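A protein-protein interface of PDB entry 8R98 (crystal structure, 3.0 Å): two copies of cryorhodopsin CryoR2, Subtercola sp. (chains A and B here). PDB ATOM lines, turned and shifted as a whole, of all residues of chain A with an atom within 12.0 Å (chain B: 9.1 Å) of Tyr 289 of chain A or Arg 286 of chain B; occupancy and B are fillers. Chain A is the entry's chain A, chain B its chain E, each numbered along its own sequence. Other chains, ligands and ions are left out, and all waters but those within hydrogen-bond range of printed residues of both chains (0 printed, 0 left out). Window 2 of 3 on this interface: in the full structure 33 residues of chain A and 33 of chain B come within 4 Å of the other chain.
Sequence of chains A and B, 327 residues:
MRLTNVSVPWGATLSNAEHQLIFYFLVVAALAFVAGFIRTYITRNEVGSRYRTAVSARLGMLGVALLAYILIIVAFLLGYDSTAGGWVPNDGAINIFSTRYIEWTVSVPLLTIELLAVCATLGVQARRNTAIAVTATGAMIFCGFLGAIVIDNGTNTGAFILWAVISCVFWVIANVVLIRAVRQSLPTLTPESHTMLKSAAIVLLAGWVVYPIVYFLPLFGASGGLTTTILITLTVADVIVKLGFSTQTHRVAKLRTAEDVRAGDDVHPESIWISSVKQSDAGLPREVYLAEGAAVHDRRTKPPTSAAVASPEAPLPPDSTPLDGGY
Leu 284 of chain B touches its own counterpart, Leu 284 of chain A. Glu 287 of chain A touches Leu 284 of chain B, but with the chains exchanged Leu 284 of chain A does not touch Glu 287 of chain B (7.5 Å). Glu 287 of chain A touches Pro 285 of chain B, but with the chains exchanged Pro 285 of chain A does not touch Glu 287 of chain B (8.6 Å). Tyr 289 of chain A touches Arg 286 of chain B, but with the chains exchanged Arg 286 of chain A does not touch Tyr 289 of chain B (15.1 Å). Of the 15 pairs that touch across the chains among the printed residues, 2 have their exchanged pair printed and touching as well.
Of the 7 printed residues of chain A, 7 touch a printed residue of chain B. Hydrophobic or aromatic side chains of chain A within 4 Å of the printed part of chain B: Leu 284, Pro 285, Tyr 289 and Leu 290. Of the 14 printed residues of chain B, 9 touch a printed residue of chain A. Hydrophobic or aromatic side chains of chain B that line the printed part of chain A: Leu 284. Among the printed residues, 15 pairs touch across the chains. Among the printed residues, no Asp or Glu carboxylate lies within 4 Å of a Lys or Arg side-chain nitrogen of the other chain.
The side-chain carboxylate (OE1) of Glu 287 of chain A lies within hydrogen-bond range of the backbone NH (N) of Glu 287 of chain B (3.1 Å). The backbone NH (N) of Val 288 of chain A is in hydrogen-bond range of the backbone carbonyl oxygen (O) of Leu 284 of chain B (2.8 Å).
Among the printed residues, merely in contact across the chains: Pro 285 of chain A with Leu 284 of chain B (3.1 Å), Glu 287 of chain A with Leu 284 of chain B (3.2 Å), Leu 290 of chain A with Gly 264 of chain B (3.3 Å), Arg 286 of chain A with Leu 284 of chain B (3.6 Å), Val 288 of chain A with Arg 286 of chain B (3.6 Å), Leu 290 of chain A with Asp 266 of chain B (3.6 Å), Glu 287 of chain A with Arg 286 of chain B (3.7 Å), Leu 290 of chain A with Val 267 of chain B (3.8 Å), Leu 290 of chain A with Asp 265 of chain B (3.9 Å), Tyr 289 of chain A with Arg 286 of chain B (3.9 Å), Pro 285 of chain A with Gly 283 of chain B (3.9 Å), Glu 287 of chain A with Pro 285 of chain B (3.9 Å) and Leu 284 of chain A with Leu 284 of chain B (3.9 Å).
Of the printed residues of chain B, Tyr 289 of chain A touches Arg 286. Arg 286 of chain B touches just these residues of chain A: Glu 287, Val 288 and Tyr 289. Glu 287 of chain B touches just one residue of chain A: Glu 287 (3.0 Å). No residue of chain A comes within 4 Å of Val 288 of chain B. Printed residues of chain B within 4 Å of Glu 287 of chain A: Leu 284, Pro 285, Arg 286 and Glu 287. Printed residues of chain A within 4 Å of Asp 266 of chain B: Leu 290. Val 261 of chain B touches none of the printed residues of chain A. The nearest residue of chain B that does not touch Tyr 289 of chain A is Gly 264 of chain B (5.5 Å). The nearest printed residue of chain A that does not touch Val 267 of chain B is Val 288 of chain A (4.7 Å).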
ATOM      1  N   LEU A 284       6.271  25.258  38.876  1.00  0.00           N
ATOM      2  CA  LEU A 284       5.839  25.147  37.459  1.00  0.00           C
ATOM      3  C   LEU A 284       6.865  24.327  36.684  1.00  0.00           C
ATOM      4  O   LEU A 284       8.062  24.411  36.944  1.00  0.00           O
ATOM      5  CB  LEU A 284       5.672  26.546  36.859  1.00  0.00           C
ATOM      6  CG  LEU A 284       4.409  27.290  37.285  1.00  0.00           C
ATOM      7  CD1 LEU A 284       4.278  28.600  36.522  1.00  0.00           C
ATOM      8  CD2 LEU A 284       3.173  26.426  37.075  1.00  0.00           C
ATOM      9  N   PRO A 285       6.415  23.504  35.712  1.00  0.00           N
ATOM     10  CA  PRO A 285       7.323  22.688  34.911  1.00  0.00           C
ATOM     11  C   PRO A 285       8.255  23.571  34.068  1.00  0.00           C
ATOM     12  O   PRO A 285       7.846  24.652  33.691  1.00  0.00           O
ATOM     13  CB  PRO A 285       6.397  21.852  34.010  1.00  0.00           C
ATOM     14  CG  PRO A 285       5.022  21.963  34.648  1.00  0.00           C
ATOM     15  CD  PRO A 285       5.006  23.305  35.345  1.00  0.00           C
ATOM     16  N   ARG A 286       9.474  23.091  33.807  1.00  0.00           N
ATOM     17  CA  ARG A 286      10.487  23.793  32.973  1.00  0.00           C
ATOM     18  C   ARG A 286       9.962  23.946  31.541  1.00  0.00           C
ATOM     19  O   ARG A 286       9.472  22.941  30.985  1.00  0.00           O
ATOM     20  CB  ARG A 286      11.809  23.019  32.977  1.00  0.00           C
ATOM     21  CG  ARG A 286      11.671  21.551  32.595  1.00  0.00           C
ATOM     22  CD  ARG A 286      12.109  21.273  31.169  1.00  0.00           C
ATOM     23  N   GLU A 287      10.058  25.156  30.975  1.00  0.00           N
ATOM     24  CA  GLU A 287       9.644  25.467  29.579  1.00  0.00           C
ATOM     25  C   GLU A 287      10.435  24.564  28.627  1.00  0.00           C
ATOM     26  O   GLU A 287      11.660  24.437  28.822  1.00  0.00           O
ATOM     27  CB  GLU A 287       9.876  26.942  29.249  1.00  0.00           C
ATOM     28  CG  GLU A 287       8.959  27.887  30.001  1.00  0.00           C
ATOM     29  CD  GLU A 287       9.080  29.344  29.593  1.00  0.00           C
ATOM     30  OE1 GLU A 287       9.694  29.611  28.541  1.00  0.00           O
ATOM     31  OE2 GLU A 287       8.564  30.209  30.330  1.00  0.00           O
ATOM     32  N   VAL A 288       9.760  23.968  27.640  1.00  0.00           N
ATOM     33  CA  VAL A 288      10.369  22.990  26.691  1.00  0.00           C
ATOM     34  C   VAL A 288      10.268  23.523  25.258  1.00  0.00           C
ATOM     35  O   VAL A 288       9.192  24.021  24.879  1.00  0.00           O
ATOM     36  CB  VAL A 288       9.706  21.605  26.822  1.00  0.00           C
ATOM     37  CG1 VAL A 288      10.291  20.600  25.841  1.00  0.00           C
ATOM     38  CG2 VAL A 288       9.797  21.075  28.244  1.00  0.00           C
ATOM     39  N   TYR A 289      11.369  23.416  24.508  1.00  0.00           N
ATOM     40  CA  TYR A 289      11.486  23.778  23.071  1.00  0.00           C
ATOM     41  C   TYR A 289      11.282  22.500  22.246  1.00  0.00           C
ATOM     42  O   TYR A 289      11.821  21.448  22.643  1.00  0.00           O
ATOM     43  CB  TYR A 289      12.850  24.409  22.776  1.00  0.00           C
ATOM     44  CG  TYR A 289      13.301  25.451  23.770  1.00  0.00           C
ATOM     45  CD1 TYR A 289      12.968  26.787  23.616  1.00  0.00           C
ATOM     46  CD2 TYR A 289      14.065  25.099  24.871  1.00  0.00           C
ATOM     47  CE1 TYR A 289      13.380  27.745  24.527  1.00  0.00           C
ATOM     48  CE2 TYR A 289      14.484  26.045  25.793  1.00  0.00           C
ATOM     49  CZ  TYR A 289      14.141  27.373  25.620  1.00  0.00           C
ATOM     50  OH  TYR A 289      14.549  28.312  26.522  1.00  0.00           O
ATOM     51  N   LEU A 290      10.539  22.585  21.139  1.00  0.00           N
ATOM     52  CA  LEU A 290      10.190  21.414  20.286  1.00  0.00           C
ATOM     53  C   LEU A 290      10.821  21.569  18.897  1.00  0.00           C
ATOM     54  O   LEU A 290      11.124  22.674  18.459  1.00  0.00           O
ATOM     55  CB  LEU A 290       8.664  21.305  20.193  1.00  0.00           C
ATOM     56  CG  LEU A 290       7.928  21.254  21.533  1.00  0.00           C
ATOM     57  CD1 LEU A 290       6.426  21.147  21.326  1.00  0.00           C
ATOM     58  CD2 LEU A 290       8.431  20.102  22.391  1.00  0.00           C
ATOM     59  N   VAL B 261       5.024  13.536  23.662  1.00  0.00           N
ATOM     60  CA  VAL B 261       5.794  14.346  24.653  1.00  0.00           C
ATOM     61  C   VAL B 261       7.250  13.867  24.653  1.00  0.00           C
ATOM     62  O   VAL B 261       8.144  14.702  24.399  1.00  0.00           O
ATOM     63  CB  VAL B 261       5.179  14.263  26.063  1.00  0.00           C
ATOM     64  CG1 VAL B 261       6.054  14.948  27.101  1.00  0.00           C
ATOM     65  CG2 VAL B 261       3.767  14.823  26.094  1.00  0.00           C
ATOM     66  N   ARG B 262       7.470  12.574  24.918  1.00  0.00           N
ATOM     67  CA  ARG B 262       8.828  11.960  24.959  1.00  0.00           C
ATOM     68  C   ARG B 262       9.548  12.225  23.630  1.00  0.00           C
ATOM     69  O   ARG B 262      10.714  12.670  23.662  1.00  0.00           O
ATOM     70  CB  ARG B 262       8.751  10.456  25.246  1.00  0.00           C
ATOM     71  CG  ARG B 262       8.309  10.109  26.660  1.00  0.00           C
ATOM     72  CD  ARG B 262       8.606   8.664  27.025  1.00  0.00           C
ATOM     73  NE  ARG B 262       7.969   7.703  26.135  1.00  0.00           N
ATOM     74  CZ  ARG B 262       6.789   7.132  26.355  1.00  0.00           C
ATOM     75  NH1 ARG B 262       6.099   7.424  27.445  1.00  0.00           N
ATOM     76  NH2 ARG B 262       6.304   6.265  25.485  1.00  0.00           N
ATOM     77  N   ALA B 263       8.867  11.969  22.509  1.00  0.00           N
ATOM     78  CA  ALA B 263       9.392  12.126  21.133  1.00  0.00           C
ATOM     79  C   ALA B 263       9.747  13.592  20.867  1.00  0.00           C
ATOM     80  O   ALA B 263      10.520  13.846  19.922  1.00  0.00           O
ATOM     81  CB  ALA B 263       8.377  11.624  20.136  1.00  0.00           C
ATOM     82  N   GLY B 264       9.186  14.515  21.653  1.00  0.00           N
ATOM     83  CA  GLY B 264       9.418  15.964  21.499  1.00  0.00           C
ATOM     84  C   GLY B 264       8.508  16.578  20.446  1.00  0.00           C
ATOM     85  O   GLY B 264       8.749  17.736  20.055  1.00  0.00           O
ATOM     86  N   ASP B 265       7.497  15.828  19.996  1.00  0.00           N
ATOM     87  CA  ASP B 265       6.502  16.295  18.993  1.00  0.00           C
ATOM     88  C   ASP B 265       5.616  17.385  19.614  1.00  0.00           C
ATOM     89  O   ASP B 265       5.304  18.352  18.898  1.00  0.00           O
ATOM     90  CB  ASP B 265       5.674  15.133  18.436  1.00  0.00           C
ATOM     91  CG  ASP B 265       6.504  14.114  17.675  1.00  0.00           C
ATOM     92  OD1 ASP B 265       7.731  14.321  17.566  1.00  0.00           O
ATOM     93  OD2 ASP B 265       5.918  13.122  17.197  1.00  0.00           O
ATOM     94  N   ASP B 266       5.230  17.252  20.888  1.00  0.00           N
ATOM     95  CA  ASP B 266       4.333  18.227  21.566  1.00  0.00           C
ATOM     96  C   ASP B 266       4.666  18.301  23.061  1.00  0.00           C
ATOM     97  O   ASP B 266       5.419  17.436  23.550  1.00  0.00           O
ATOM     98  CB  ASP B 266       2.866  17.858  21.335  1.00  0.00           C
ATOM     99  CG  ASP B 266       1.891  18.985  21.638  1.00  0.00           C
ATOM    100  OD1 ASP B 266       0.676  18.709  21.691  1.00  0.00           O
ATOM    101  OD2 ASP B 266       2.355  20.130  21.801  1.00  0.00           O
ATOM    102  N   VAL B 267       4.115  19.301  23.756  1.00  0.00           N
ATOM    103  CA  VAL B 267       4.320  19.527  25.219  1.00  0.00           C
ATOM    104  C   VAL B 267       2.974  19.388  25.939  1.00  0.00           C
ATOM    105  O   VAL B 267       1.973  19.928  25.430  1.00  0.00           O
ATOM    106  CB  VAL B 267       4.958  20.903  25.492  1.00  0.00           C
ATOM    107  CG1 VAL B 267       4.265  22.019  24.722  1.00  0.00           C
ATOM    108  CG2 VAL B 267       4.990  21.227  26.979  1.00  0.00           C
ATOM    109  N   GLY B 283       5.646  19.358  31.133  1.00  0.00           N
ATOM    110  CA  GLY B 283       6.336  20.328  30.260  1.00  0.00           C
ATOM    111  C   GLY B 283       5.474  21.549  30.015  1.00  0.00           C
ATOM    112  O   GLY B 283       4.238  21.390  29.943  1.00  0.00           O
ATOM    113  N   LEU B 284       6.089  22.729  29.920  1.00  0.00           N
ATOM    114  CA  LEU B 284       5.369  23.995  29.625  1.00  0.00           C
ATOM    115  C   LEU B 284       5.881  24.547  28.300  1.00  0.00           C
ATOM    116  O   LEU B 284       7.075  24.479  28.016  1.00  0.00           O
ATOM    117  CB  LEU B 284       5.573  24.997  30.763  1.00  0.00           C
ATOM    118  CG  LEU B 284       4.902  24.650  32.091  1.00  0.00           C
ATOM    119  CD1 LEU B 284       4.998  25.822  33.057  1.00  0.00           C
ATOM    120  CD2 LEU B 284       3.444  24.259  31.892  1.00  0.00           C
ATOM    121  N   PRO B 285       4.982  25.078  27.443  1.00  0.00           N
ATOM    122  CA  PRO B 285       5.380  25.624  26.146  1.00  0.00           C
ATOM    123  C   PRO B 285       6.322  26.825  26.330  1.00  0.00           C
ATOM    124  O   PRO B 285       6.164  27.539  27.305  1.00  0.00           O
ATOM    125  CB  PRO B 285       4.060  26.057  25.489  1.00  0.00           C
ATOM    126  CG  PRO B 285       2.973  25.354  26.289  1.00  0.00           C
ATOM    127  CD  PRO B 285       3.537  25.185  27.684  1.00  0.00           C
ATOM    128  N   ARG B 286       7.273  27.013  25.410  1.00  0.00           N
ATOM    129  CA  ARG B 286       8.267  28.120  25.480  1.00  0.00           C
ATOM    130  C   ARG B 286       7.548  29.462  25.299  1.00  0.00           C
ATOM    131  O   ARG B 286       6.745  29.568  24.358  1.00  0.00           O
ATOM    132  CB  ARG B 286       9.349  27.939  24.413  1.00  0.00           C
ATOM    133  N   GLU B 287       7.815  30.437  26.176  1.00  0.00           N
ATOM    134  CA  GLU B 287       7.249  31.812  26.083  1.00  0.00           C
ATOM    135  C   GLU B 287       7.713  32.422  24.757  1.00  0.00           C
ATOM    136  O   GLU B 287       8.904  32.277  24.434  1.00  0.00           O
ATOM    137  CB  GLU B 287       7.673  32.663  27.279  1.00  0.00           C
ATOM    138  CG  GLU B 287       7.025  32.228  28.581  1.00  0.00           C
ATOM    139  CD  GLU B 287       7.513  32.964  29.816  1.00  0.00           C
ATOM    140  OE1 GLU B 287       8.431  33.797  29.684  1.00  0.00           O
ATOM    141  OE2 GLU B 287       6.973  32.700  30.906  1.00  0.00           O
ATOM    142  N   VAL B 288       6.806  33.069  24.021  1.00  0.00           N
ATOM    143  CA  VAL B 288       7.069  33.600  22.650  1.00  0.00           C
ATOM    144  C   VAL B 288       6.842  35.116  22.623  1.00  0.00           C
ATOM    145  O   VAL B 288       5.843  35.573  23.209  1.00  0.00           O
ATOM    146  CB  VAL B 288       6.178  32.887  21.611  1.00  0.00           C
ATOM    147  CG1 VAL B 288       6.403  33.419  20.205  1.00  0.00           C
ATOM    148  CG2 VAL B 288       6.373  31.380  21.634  1.00  0.00           C
ATOM    149  N   TYR B 289       7.741  35.850  21.954  1.00  0.00           N
ATOM    150  CA  TYR B 289       7.647  37.308  21.675  1.00  0.00           C
ATOM    151  C   TYR B 289       6.937  37.531  20.331  1.00  0.00           C
ATOM    152  O   TYR B 289       7.213  36.781  19.375  1.00  0.00           O
ATOM    153  CB  TYR B 289       9.040  37.938  21.621  1.00  0.00           C
ATOM    154  CG  TYR B 289       9.691  38.187  22.956  1.00  0.00           C
ATOM    155  CD1 TYR B 289       9.557  39.410  23.593  1.00  0.00           C
ATOM    156  CD2 TYR B 289      10.457  37.214  23.576  1.00  0.00           C
ATOM    157  CE1 TYR B 289      10.159  39.658  24.814  1.00  0.00           C
ATOM    158  CE2 TYR B 289      11.066  37.446  24.798  1.00  0.00           C
ATOM    159  CZ  TYR B 289      10.916  38.672  25.421  1.00  0.00           C
ATOM    160  OH  TYR B 289      11.511  38.910  26.626  1.00  0.00           O
